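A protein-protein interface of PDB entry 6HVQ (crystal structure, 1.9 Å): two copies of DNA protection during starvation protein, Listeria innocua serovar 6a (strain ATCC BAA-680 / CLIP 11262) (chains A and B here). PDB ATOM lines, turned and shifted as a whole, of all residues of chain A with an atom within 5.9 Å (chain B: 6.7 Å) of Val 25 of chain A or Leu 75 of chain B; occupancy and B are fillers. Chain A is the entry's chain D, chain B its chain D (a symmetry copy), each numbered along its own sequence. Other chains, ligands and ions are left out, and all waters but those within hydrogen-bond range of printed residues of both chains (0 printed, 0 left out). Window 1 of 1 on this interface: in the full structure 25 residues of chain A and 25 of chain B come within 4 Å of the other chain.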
ATOM      1  N   ALA A  18      11.907 -17.893  -6.055  1.00  0.00           N
ATOM      2  CA  ALA A  18      10.587 -18.420  -5.708  1.00  0.00           C
ATOM      3  C   ALA A  18       9.503 -17.352  -5.852  1.00  0.00           C
ATOM      4  O   ALA A  18       8.472 -17.567  -6.523  1.00  0.00           O
ATOM      5  CB  ALA A  18      10.620 -18.977  -4.283  1.00  0.00           C
ATOM      6  N   LEU A  20       9.371 -14.679  -7.621  1.00  0.00           N
ATOM      7  CA  LEU A  20       9.116 -14.230  -8.984  1.00  0.00           C
ATOM      8  C   LEU A  20       8.380 -15.277  -9.812  1.00  0.00           C
ATOM      9  O   LEU A  20       7.596 -14.906 -10.695  1.00  0.00           O
ATOM     10  CB  LEU A  20      10.430 -13.830  -9.652  1.00  0.00           C
ATOM     11  CG  LEU A  20      11.016 -12.528  -9.086  1.00  0.00           C
ATOM     12  CD1 LEU A  20      12.468 -12.349  -9.496  1.00  0.00           C
ATOM     13  CD2 LEU A  20      10.196 -11.323  -9.532  1.00  0.00           C
ATOM     14  N   ASN A  21       8.605 -16.578  -9.558  1.00  0.00           N
ATOM     15  CA  ASN A  21       7.799 -17.583 -10.255  1.00  0.00           C
ATOM     16  C   ASN A  21       6.335 -17.529  -9.818  1.00  0.00           C
ATOM     17  O   ASN A  21       5.414 -17.564 -10.662  1.00  0.00           O
ATOM     18  CB  ASN A  21       8.382 -18.983 -10.036  1.00  0.00           C
ATOM     19  CG  ASN A  21       9.462 -19.321 -11.047  1.00  0.00           C
ATOM     20  OD1 ASN A  21       9.162 -19.778 -12.148  1.00  0.00           O
ATOM     21  ND2 ASN A  21      10.719 -19.091 -10.687  1.00  0.00           N
ATOM     22  N   VAL A  22       6.093 -17.396  -8.510  1.00  0.00           N
ATOM     23  CA  VAL A  22       4.713 -17.216  -8.054  1.00  0.00           C
ATOM     24  C   VAL A  22       4.107 -15.967  -8.693  1.00  0.00           C
ATOM     25  O   VAL A  22       2.937 -15.959  -9.111  1.00  0.00           O
ATOM     26  CB  VAL A  22       4.658 -17.166  -6.515  1.00  0.00           C
ATOM     27  CG1 VAL A  22       3.228 -16.929  -6.018  1.00  0.00           C
ATOM     28  CG2 VAL A  22       5.203 -18.460  -5.927  1.00  0.00           C
ATOM     29  N   PHE A  23       4.901 -14.898  -8.799  1.00  0.00           N
ATOM     30  CA  PHE A  23       4.382 -13.632  -9.304  1.00  0.00           C
ATOM     31  C   PHE A  23       4.007 -13.726 -10.776  1.00  0.00           C
ATOM     32  O   PHE A  23       2.947 -13.234 -11.179  1.00  0.00           O
ATOM     33  CB  PHE A  23       5.406 -12.520  -9.089  1.00  0.00           C
ATOM     34  CG  PHE A  23       4.894 -11.133  -9.413  1.00  0.00           C
ATOM     35  CD1 PHE A  23       3.562 -10.796  -9.228  1.00  0.00           C
ATOM     36  CD2 PHE A  23       5.763 -10.161  -9.885  1.00  0.00           C
ATOM     37  CE1 PHE A  23       3.106  -9.516  -9.516  1.00  0.00           C
ATOM     38  CE2 PHE A  23       5.318  -8.884 -10.168  1.00  0.00           C
ATOM     39  CZ  PHE A  23       3.984  -8.560  -9.984  1.00  0.00           C
ATOM     40  N   THR A  24       4.857 -14.337 -11.607  1.00  0.00           N
ATOM     41  CA  THR A  24       4.517 -14.409 -13.024  1.00  0.00           C
ATOM     42  C   THR A  24       3.269 -15.255 -13.242  1.00  0.00           C
ATOM     43  O   THR A  24       2.425 -14.925 -14.093  1.00  0.00           O
ATOM     44  CB  THR A  24       5.689 -14.950 -13.846  1.00  0.00           C
ATOM     45  OG1 THR A  24       6.185 -16.158 -13.253  1.00  0.00           O
ATOM     46  CG2 THR A  24       6.795 -13.909 -13.942  1.00  0.00           C
ATOM     47  N   VAL A  25       3.112 -16.333 -12.470  1.00  0.00           N
ATOM     48  CA  VAL A  25       1.875 -17.101 -12.595  1.00  0.00           C
ATOM     49  C   VAL A  25       0.672 -16.242 -12.201  1.00  0.00           C
ATOM     50  O   VAL A  25      -0.385 -16.296 -12.848  1.00  0.00           O
ATOM     51  CB  VAL A  25       1.969 -18.402 -11.777  1.00  0.00           C
ATOM     52  CG1 VAL A  25       0.618 -19.124 -11.733  1.00  0.00           C
ATOM     53  CG2 VAL A  25       3.030 -19.308 -12.385  1.00  0.00           C
ATOM     54  N   LYS A  26       0.820 -15.406 -11.162  1.00  0.00           N
ATOM     55  CA  LYS A  26      -0.271 -14.502 -10.792  1.00  0.00           C
ATOM     56  C   LYS A  26      -0.591 -13.523 -11.924  1.00  0.00           C
ATOM     57  O   LYS A  26      -1.761 -13.184 -12.166  1.00  0.00           O
ATOM     58  CB  LYS A  26       0.087 -13.733  -9.520  1.00  0.00           C
ATOM     59  CG  LYS A  26      -1.027 -12.812  -9.025  1.00  0.00           C
ATOM     60  CD  LYS A  26      -0.551 -11.876  -7.924  1.00  0.00           C
ATOM     61  CE  LYS A  26      -0.253 -12.596  -6.618  1.00  0.00           C
ATOM     62  NZ  LYS A  26      -1.492 -13.077  -5.958  1.00  0.00           N
ATOM     63  N   ILE A  27       0.444 -13.018 -12.594  1.00  0.00           N
ATOM     64  CA  ILE A  27       0.241 -12.100 -13.710  1.00  0.00           C
ATOM     65  C   ILE A  27      -0.560 -12.775 -14.812  1.00  0.00           C
ATOM     66  O   ILE A  27      -1.426 -12.150 -15.434  1.00  0.00           O
ATOM     67  CB  ILE A  27       1.596 -11.567 -14.211  1.00  0.00           C
ATOM     68  CG1 ILE A  27       2.200 -10.646 -13.140  1.00  0.00           C
ATOM     69  CG2 ILE A  27       1.442 -10.827 -15.537  1.00  0.00           C
ATOM     70  CD1 ILE A  27       3.671 -10.301 -13.361  1.00  0.00           C
ATOM     71  N   HIS A  28      -0.278 -14.056 -15.085  1.00  0.00           N
ATOM     72  CA  HIS A  28      -1.093 -14.780 -16.062  1.00  0.00           C
ATOM     73  C   HIS A  28      -2.533 -14.949 -15.582  1.00  0.00           C
ATOM     74  O   HIS A  28      -3.469 -14.871 -16.388  1.00  0.00           O
ATOM     75  CB  HIS A  28      -0.485 -16.147 -16.370  1.00  0.00           C
ATOM     76  CG  HIS A  28       0.380 -16.168 -17.593  1.00  0.00           C
ATOM     77  ND1 HIS A  28       0.391 -15.148 -18.522  1.00  0.00           N
ATOM     78  CD2 HIS A  28       1.257 -17.095 -18.043  1.00  0.00           C
ATOM     79  CE1 HIS A  28       1.246 -15.443 -19.485  1.00  0.00           C
ATOM     80  NE2 HIS A  28       1.785 -16.619 -19.217  1.00  0.00           N
ATOM     81  N   GLN A  29      -2.732 -15.231 -14.291  1.00  0.00           N
ATOM     82  CA  GLN A  29      -4.088 -15.291 -13.744  1.00  0.00           C
ATOM     83  C   GLN A  29      -4.867 -14.014 -14.057  1.00  0.00           C
ATOM     84  O   GLN A  29      -6.012 -14.058 -14.531  1.00  0.00           O
ATOM     85  CB  GLN A  29      -4.028 -15.520 -12.230  1.00  0.00           C
ATOM     86  CG  GLN A  29      -5.388 -15.556 -11.527  1.00  0.00           C
ATOM     87  CD  GLN A  29      -5.271 -15.733 -10.020  1.00  0.00           C
ATOM     88  OE1 GLN A  29      -5.173 -14.758  -9.273  1.00  0.00           O
ATOM     89  NE2 GLN A  29      -5.299 -16.976  -9.565  1.00  0.00           N
ATOM     90  N   ILE A  30      -4.259 -12.860 -13.784  1.00  0.00           N
ATOM     91  CA  ILE A  30      -4.924 -11.583 -14.036  1.00  0.00           C
ATOM     92  C   ILE A  30      -5.163 -11.396 -15.529  1.00  0.00           C
ATOM     93  O   ILE A  30      -6.248 -10.987 -15.962  1.00  0.00           O
ATOM     94  CB  ILE A  30      -4.094 -10.433 -13.438  1.00  0.00           C
ATOM     95  CG1 ILE A  30      -4.045 -10.562 -11.912  1.00  0.00           C
ATOM     96  CG2 ILE A  30      -4.679  -9.087 -13.814  1.00  0.00           C
ATOM     97  CD1 ILE A  30      -3.018  -9.676 -11.234  1.00  0.00           C
ATOM     98  N   TRP A  32      -5.628 -13.610 -17.805  1.00  0.00           N
ATOM     99  CA  TRP A  32      -6.655 -14.513 -18.313  1.00  0.00           C
ATOM    100  C   TRP A  32      -8.053 -14.146 -17.824  1.00  0.00           C
ATOM    101  O   TRP A  32      -9.012 -14.188 -18.607  1.00  0.00           O
ATOM    102  CB  TRP A  32      -6.335 -15.953 -17.899  1.00  0.00           C
ATOM    103  CG  TRP A  32      -5.146 -16.564 -18.591  1.00  0.00           C
ATOM    104  CD1 TRP A  32      -4.650 -16.230 -19.818  1.00  0.00           C
ATOM    105  CD2 TRP A  32      -4.307 -17.614 -18.092  1.00  0.00           C
ATOM    106  NE1 TRP A  32      -3.559 -17.009 -20.116  1.00  0.00           N
ATOM    107  CE2 TRP A  32      -3.325 -17.864 -19.071  1.00  0.00           C
ATOM    108  CE3 TRP A  32      -4.291 -18.367 -16.914  1.00  0.00           C
ATOM    109  CZ2 TRP A  32      -2.333 -18.833 -18.906  1.00  0.00           C
ATOM    110  CZ3 TRP A  32      -3.309 -19.329 -16.753  1.00  0.00           C
ATOM    111  CH2 TRP A  32      -2.341 -19.551 -17.741  1.00  0.00           C
ATOM    112  N   TYR A  50       4.676  -9.725 -17.499  1.00  0.00           N
ATOM    113  CA  TYR A  50       5.086 -11.127 -17.514  1.00  0.00           C
ATOM    114  C   TYR A  50       6.494 -11.262 -18.070  1.00  0.00           C
ATOM    115  O   TYR A  50       7.341 -11.963 -17.497  1.00  0.00           O
ATOM    116  CB  TYR A  50       4.095 -11.951 -18.339  1.00  0.00           C
ATOM    117  CG  TYR A  50       4.323 -13.449 -18.251  1.00  0.00           C
ATOM    118  CD1 TYR A  50       3.809 -14.183 -17.195  1.00  0.00           C
ATOM    119  CD2 TYR A  50       5.039 -14.122 -19.232  1.00  0.00           C
ATOM    120  CE1 TYR A  50       4.010 -15.547 -17.105  1.00  0.00           C
ATOM    121  CE2 TYR A  50       5.249 -15.488 -19.154  1.00  0.00           C
ATOM    122  CZ  TYR A  50       4.732 -16.196 -18.086  1.00  0.00           C
ATOM    123  OH  TYR A  50       4.931 -17.555 -17.998  1.00  0.00           O
ATOM    124  N   THR A  74      11.827 -26.029  -9.119  1.00  0.00           N
ATOM    125  CA  THR A  74      10.601 -26.816  -9.198  1.00  0.00           C
ATOM    126  C   THR A  74       9.468 -26.021  -8.563  1.00  0.00           C
ATOM    127  O   THR A  74       9.699 -25.163  -7.706  1.00  0.00           O
ATOM    128  CB  THR A  74      10.737 -28.167  -8.488  1.00  0.00           C
ATOM    129  OG1 THR A  74      11.036 -27.946  -7.107  1.00  0.00           O
ATOM    130  CG2 THR A  74      11.839 -29.003  -9.123  1.00  0.00           C
ATOM    131  N   LEU A  75       8.233 -26.312  -8.980  1.00  0.00           N
ATOM    132  CA  LEU A  75       7.084 -25.645  -8.372  1.00  0.00           C
ATOM    133  C   LEU A  75       7.014 -25.916  -6.874  1.00  0.00           C
ATOM    134  O   LEU A  75       6.655 -25.027  -6.093  1.00  0.00           O
ATOM    135  CB  LEU A  75       5.787 -26.084  -9.050  1.00  0.00           C
ATOM    136  CG  LEU A  75       5.456 -25.426 -10.395  1.00  0.00           C
ATOM    137  CD1 LEU A  75       6.456 -25.810 -11.465  1.00  0.00           C
ATOM    138  CD2 LEU A  75       4.046 -25.802 -10.829  1.00  0.00           C
ATOM    139  N   PHE A  78       9.359 -23.571  -5.158  1.00  0.00           N
ATOM    140  CA  PHE A  78       8.837 -22.209  -5.211  1.00  0.00           C
ATOM    141  C   PHE A  78       7.757 -22.010  -4.154  1.00  0.00           C
ATOM    142  O   PHE A  78       7.780 -21.031  -3.396  1.00  0.00           O
ATOM    143  CB  PHE A  78       8.276 -21.901  -6.604  1.00  0.00           C
ATOM    144  CG  PHE A  78       9.274 -22.038  -7.730  1.00  0.00           C
ATOM    145  CD1 PHE A  78      10.637 -21.910  -7.506  1.00  0.00           C
ATOM    146  CD2 PHE A  78       8.833 -22.280  -9.027  1.00  0.00           C
ATOM    147  CE1 PHE A  78      11.537 -22.035  -8.556  1.00  0.00           C
ATOM    148  CE2 PHE A  78       9.725 -22.402 -10.071  1.00  0.00           C
ATOM    149  CZ  PHE A  78      11.081 -22.282  -9.837  1.00  0.00           C
ATOM    150  N   LEU A  79       6.809 -22.947  -4.080  1.00  0.00           N
ATOM    151  CA  LEU A  79       5.716 -22.835  -3.124  1.00  0.00           C
ATOM    152  C   LEU A  79       6.218 -22.932  -1.692  1.00  0.00           C
ATOM    153  O   LEU A  79       5.736 -22.212  -0.810  1.00  0.00           O
ATOM    154  CB  LEU A  79       4.678 -23.914  -3.410  1.00  0.00           C
ATOM    155  CG  LEU A  79       3.616 -23.547  -4.440  1.00  0.00           C
ATOM    156  CD1 LEU A  79       2.741 -24.745  -4.722  1.00  0.00           C
ATOM    157  CD2 LEU A  79       2.759 -22.385  -3.949  1.00  0.00           C
ATOM    158  N   GLU A  86      -0.594 -16.545  -3.368  1.00  0.00           N
ATOM    159  CA  GLU A  86      -1.465 -16.856  -4.495  1.00  0.00           C
ATOM    160  C   GLU A  86      -2.750 -17.480  -3.963  1.00  0.00           C
ATOM    161  O   GLU A  86      -2.777 -18.047  -2.869  1.00  0.00           O
ATOM    162  CB  GLU A  86      -0.784 -17.813  -5.486  1.00  0.00           C
ATOM    163  CG  GLU A  86      -0.351 -19.138  -4.857  1.00  0.00           C
ATOM    164  CD  GLU A  86       0.088 -20.173  -5.881  1.00  0.00           C
ATOM    165  OE1 GLU A  86       0.485 -19.796  -7.003  1.00  0.00           O
ATOM    166  OE2 GLU A  86       0.030 -21.379  -5.558  1.00  0.00           O
ATOM    167  N   ASN B  21       2.953 -25.734 -17.436  1.00  0.00           N
ATOM    168  CA  ASN B  21       3.666 -24.924 -16.445  1.00  0.00           C
ATOM    169  C   ASN B  21       4.775 -25.724 -15.760  1.00  0.00           C
ATOM    170  O   ASN B  21       5.913 -25.233 -15.602  1.00  0.00           O
ATOM    171  CB  ASN B  21       2.686 -24.356 -15.413  1.00  0.00           C
ATOM    172  CG  ASN B  21       2.071 -23.045 -15.865  1.00  0.00           C
ATOM    173  OD1 ASN B  21       2.659 -21.983 -15.675  1.00  0.00           O
ATOM    174  ND2 ASN B  21       0.892 -23.110 -16.473  1.00  0.00           N
ATOM    175  N   PHE B  72      -6.701 -23.457 -14.567  1.00  0.00           N
ATOM    176  CA  PHE B  72      -5.840 -23.422 -13.393  1.00  0.00           C
ATOM    177  C   PHE B  72      -4.898 -22.233 -13.517  1.00  0.00           C
ATOM    178  O   PHE B  72      -4.440 -21.910 -14.611  1.00  0.00           O
ATOM    179  CB  PHE B  72      -5.015 -24.712 -13.284  1.00  0.00           C
ATOM    180  CG  PHE B  72      -5.834 -25.967 -13.162  1.00  0.00           C
ATOM    181  CD1 PHE B  72      -6.867 -26.063 -12.249  1.00  0.00           C
ATOM    182  CD2 PHE B  72      -5.554 -27.058 -13.965  1.00  0.00           C
ATOM    183  CE1 PHE B  72      -7.613 -27.229 -12.142  1.00  0.00           C
ATOM    184  CE2 PHE B  72      -6.292 -28.227 -13.863  1.00  0.00           C
ATOM    185  CZ  PHE B  72      -7.319 -28.312 -12.954  1.00  0.00           C
ATOM    186  N   SER B  73      -4.602 -21.581 -12.389  1.00  0.00           N
ATOM    187  CA  SER B  73      -3.807 -20.358 -12.445  1.00  0.00           C
ATOM    188  C   SER B  73      -3.019 -20.122 -11.158  1.00  0.00           C
ATOM    189  O   SER B  73      -2.798 -18.968 -10.771  1.00  0.00           O
ATOM    190  CB  SER B  73      -4.710 -19.157 -12.750  1.00  0.00           C
ATOM    191  OG  SER B  73      -5.689 -18.987 -11.741  1.00  0.00           O
ATOM    192  N   THR B  74      -2.611 -21.197 -10.482  1.00  0.00           N
ATOM    193  CA  THR B  74      -1.728 -21.127  -9.324  1.00  0.00           C
ATOM    194  C   THR B  74      -0.786 -22.325  -9.355  1.00  0.00           C
ATOM    195  O   THR B  74      -1.105 -23.366  -9.935  1.00  0.00           O
ATOM    196  CB  THR B  74      -2.507 -21.126  -8.005  1.00  0.00           C
ATOM    197  OG1 THR B  74      -3.274 -22.329  -7.908  1.00  0.00           O
ATOM    198  CG2 THR B  74      -3.433 -19.920  -7.925  1.00  0.00           C
ATOM    199  N   LEU B  75       0.380 -22.177  -8.720  1.00  0.00           N
ATOM    200  CA  LEU B  75       1.312 -23.301  -8.643  1.00  0.00           C
ATOM    201  C   LEU B  75       0.683 -24.495  -7.936  1.00  0.00           C
ATOM    202  O   LEU B  75       0.917 -25.646  -8.323  1.00  0.00           O
ATOM    203  CB  LEU B  75       2.598 -22.882  -7.933  1.00  0.00           C
ATOM    204  CG  LEU B  75       3.619 -22.095  -8.763  1.00  0.00           C
ATOM    205  CD1 LEU B  75       3.083 -20.736  -9.160  1.00  0.00           C
ATOM    206  CD2 LEU B  75       4.921 -21.946  -7.987  1.00  0.00           C
ATOM    207  N   LYS B  76      -0.104 -24.246  -6.886  1.00  0.00           N
ATOM    208  CA  LYS B  76      -0.763 -25.337  -6.175  1.00  0.00           C
ATOM    209  C   LYS B  76      -1.650 -26.154  -7.110  1.00  0.00           C
ATOM    210  O   LYS B  76      -1.627 -27.391  -7.088  1.00  0.00           O
ATOM    211  CB  LYS B  76      -1.582 -24.773  -5.011  1.00  0.00           C
ATOM    212  CG  LYS B  76      -2.244 -25.827  -4.151  1.00  0.00           C
ATOM    213  CD  LYS B  76      -3.037 -25.203  -3.013  1.00  0.00           C
ATOM    214  CE  LYS B  76      -3.776 -26.259  -2.203  1.00  0.00           C
ATOM    215  NZ  LYS B  76      -4.550 -25.663  -1.085  1.00  0.00           N
ATOM    216  N   GLU B  77      -2.461 -25.479  -7.928  1.00  0.00           N
ATOM    217  CA  GLU B  77      -3.316 -26.194  -8.874  1.00  0.00           C
ATOM    218  C   GLU B  77      -2.485 -26.960  -9.900  1.00  0.00           C
ATOM    219  O   GLU B  77      -2.789 -28.118 -10.227  1.00  0.00           O
ATOM    220  CB  GLU B  77      -4.258 -25.210  -9.573  1.00  0.00           C
ATOM    221  CG  GLU B  77      -5.387 -24.682  -8.690  1.00  0.00           C
ATOM    222  CD  GLU B  77      -6.184 -23.569  -9.355  1.00  0.00           C
ATOM    223  OE1 GLU B  77      -5.584 -22.543  -9.731  1.00  0.00           O
ATOM    224  OE2 GLU B  77      -7.412 -23.726  -9.500  1.00  0.00           O
ATOM    225  N   PHE B  78      -1.421 -26.335 -10.412  1.00  0.00           N
ATOM    226  CA  PHE B  78      -0.573 -27.014 -11.387  1.00  0.00           C
ATOM    227  C   PHE B  78      -0.014 -28.304 -10.802  1.00  0.00           C
ATOM    228  O   PHE B  78      -0.078 -29.369 -11.430  1.00  0.00           O
ATOM    229  CB  PHE B  78       0.571 -26.097 -11.835  1.00  0.00           C
ATOM    230  CG  PHE B  78       0.128 -24.795 -12.462  1.00  0.00           C
ATOM    231  CD1 PHE B  78      -1.114 -24.671 -13.066  1.00  0.00           C
ATOM    232  CD2 PHE B  78       0.979 -23.695 -12.456  1.00  0.00           C
ATOM    233  CE1 PHE B  78      -1.500 -23.467 -13.639  1.00  0.00           C
ATOM    234  CE2 PHE B  78       0.599 -22.499 -13.027  1.00  0.00           C
ATOM    235  CZ  PHE B  78      -0.644 -22.382 -13.619  1.00  0.00           C
ATOM    236  N   LEU B  79       0.524 -28.227  -9.582  1.00  0.00           N
ATOM    237  CA  LEU B  79       1.112 -29.397  -8.946  1.00  0.00           C
ATOM    238  C   LEU B  79       0.061 -30.454  -8.643  1.00  0.00           C
ATOM    239  O   LEU B  79       0.314 -31.653  -8.804  1.00  0.00           O
ATOM    240  CB  LEU B  79       1.838 -28.974  -7.674  1.00  0.00           C
ATOM    241  CG  LEU B  79       3.285 -28.533  -7.859  1.00  0.00           C
ATOM    242  CD1 LEU B  79       3.835 -28.017  -6.551  1.00  0.00           C
ATOM    243  CD2 LEU B  79       4.146 -29.687  -8.363  1.00  0.00           C
ATOM    244  N   GLU B  80      -1.126 -30.033  -8.204  1.00  0.00           N
ATOM    245  CA  GLU B  80      -2.168 -30.999  -7.886  1.00  0.00           C
ATOM    246  C   GLU B  80      -2.682 -31.726  -9.120  1.00  0.00           C
ATOM    247  O   GLU B  80      -3.202 -32.838  -8.985  1.00  0.00           O
ATOM    248  CB  GLU B  80      -3.339 -30.312  -7.181  1.00  0.00           C
ATOM    249  CG  GLU B  80      -3.106 -30.054  -5.699  1.00  0.00           C
ATOM    250  CD  GLU B  80      -4.123 -29.090  -5.097  1.00  0.00           C
ATOM    251  OE1 GLU B  80      -4.904 -28.478  -5.861  1.00  0.00           O
ATOM    252  OE2 GLU B  80      -4.131 -28.940  -3.855  1.00  0.00           O
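Thr 24 of chain A touches none of the printed residues of chain B.
Of chain B, only Ser 73 (3.6 Å), Thr 74 (3.9 Å), Leu 75 (3.5 Å) and Phe 78 (3.6 Å) come within 4 Å of Val 25 of chain A.
Ile 30 of chain A touches none of the printed residues of chain B.
Of the printed residues of chain B, Leu 79 of chain A touches Leu 75, Lys 76 and Leu 79.
Printed residues of chain A within 4 Å of Leu 75 of chain B: Val 25, Phe 78, Leu 79 and Glu 86.
Printed residues of chain A within 4 Å of Phe 78 of chain B: Val 25 and Leu 75.
The nearest residue of chain B that does not touch Val 25 of chain A is Asn 21 of chain B (4.3 Å).
The nearest printed residue of chain A that does not touch Leu 75 of chain B is Leu 75 of chain A (4.01 Å).
Hydrophobic or aromatic side chains of chain B that line the printed part of chain A: Leu 75, Phe 78 and Leu 79.
Hydrophobic or aromatic side chains of chain A that line the printed part of chain B: Val 25, Trp 32, Leu 75, Phe 78 and Leu 79.
Along chain A the printed residues that touch a printed residue of chain B span positions 25 to 86.
OE2 of Glu 86 of chain A lies within hydrogen-bond range of N of Lys 76 of chain B (3.2 Å).
N of Leu 75 of chain B lies within hydrogen-bond range of OE1 of Glu 86 of chain A (2.9 Å).
OG of Ser 73 of chain B lies within hydrogen-bond range of NE2 of Gln 29 of chain A, at 3.0 Å.
Leu 75 of chain A touches Phe 78 of chain B, and with the chains exchanged Phe 78 of chain A touches Leu 75 of chain B.
Leu 75 of chain A touches Leu 79 of chain B, and with the chains exchanged Leu 79 of chain A touches Leu 75 of chain B.
Leu 79 of chain A touches its own counterpart, Leu 79 of chain B.
Of the 16 pairs that touch across the chains among the printed residues, 5 have their exchanged pair printed and touching as well.
Among the printed residues, merely in contact across the chains: Val 25 of chain A with Ser 73 of chain B (3.6 Å), Val 25 of chain A with Thr 74 of chain B (3.9 Å), Val 25 of chain A with Leu 75 of chain B (3.5 Å), Val 25 of chain A with Phe 78 of chain B (3.6 Å), Gln 29 of chain A with Thr 74 of chain B (3.9 Å), Trp 32 of chain A with Phe 72 of chain B (3.5 Å), Leu 75 of chain A with Phe 78 of chain B (3.6 Å), Leu 75 of chain A with Leu 79 of chain B (3.7 Å), Phe 78 of chain A with Leu 75 of chain B (3.6 Å), Leu 79 of chain A with Leu 75 of chain B (3.7 Å), Leu 79 of chain A with Lys 76 of chain B (3.6 Å), Leu 79 of chain A with Leu 79 of chain B (3.9 Å) and Glu 86 of chain A with Thr 74 of chain B (3.4 Å).
N of Ser 73 of chain B sits at hydrogen-bond distance from OE1 of Glu 77 of chain B (3.0 Å).
OE1 of Glu 77 of chain B is in hydrogen-bond range of OG1 of Thr 74 of chain B, 3.0 Å away.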
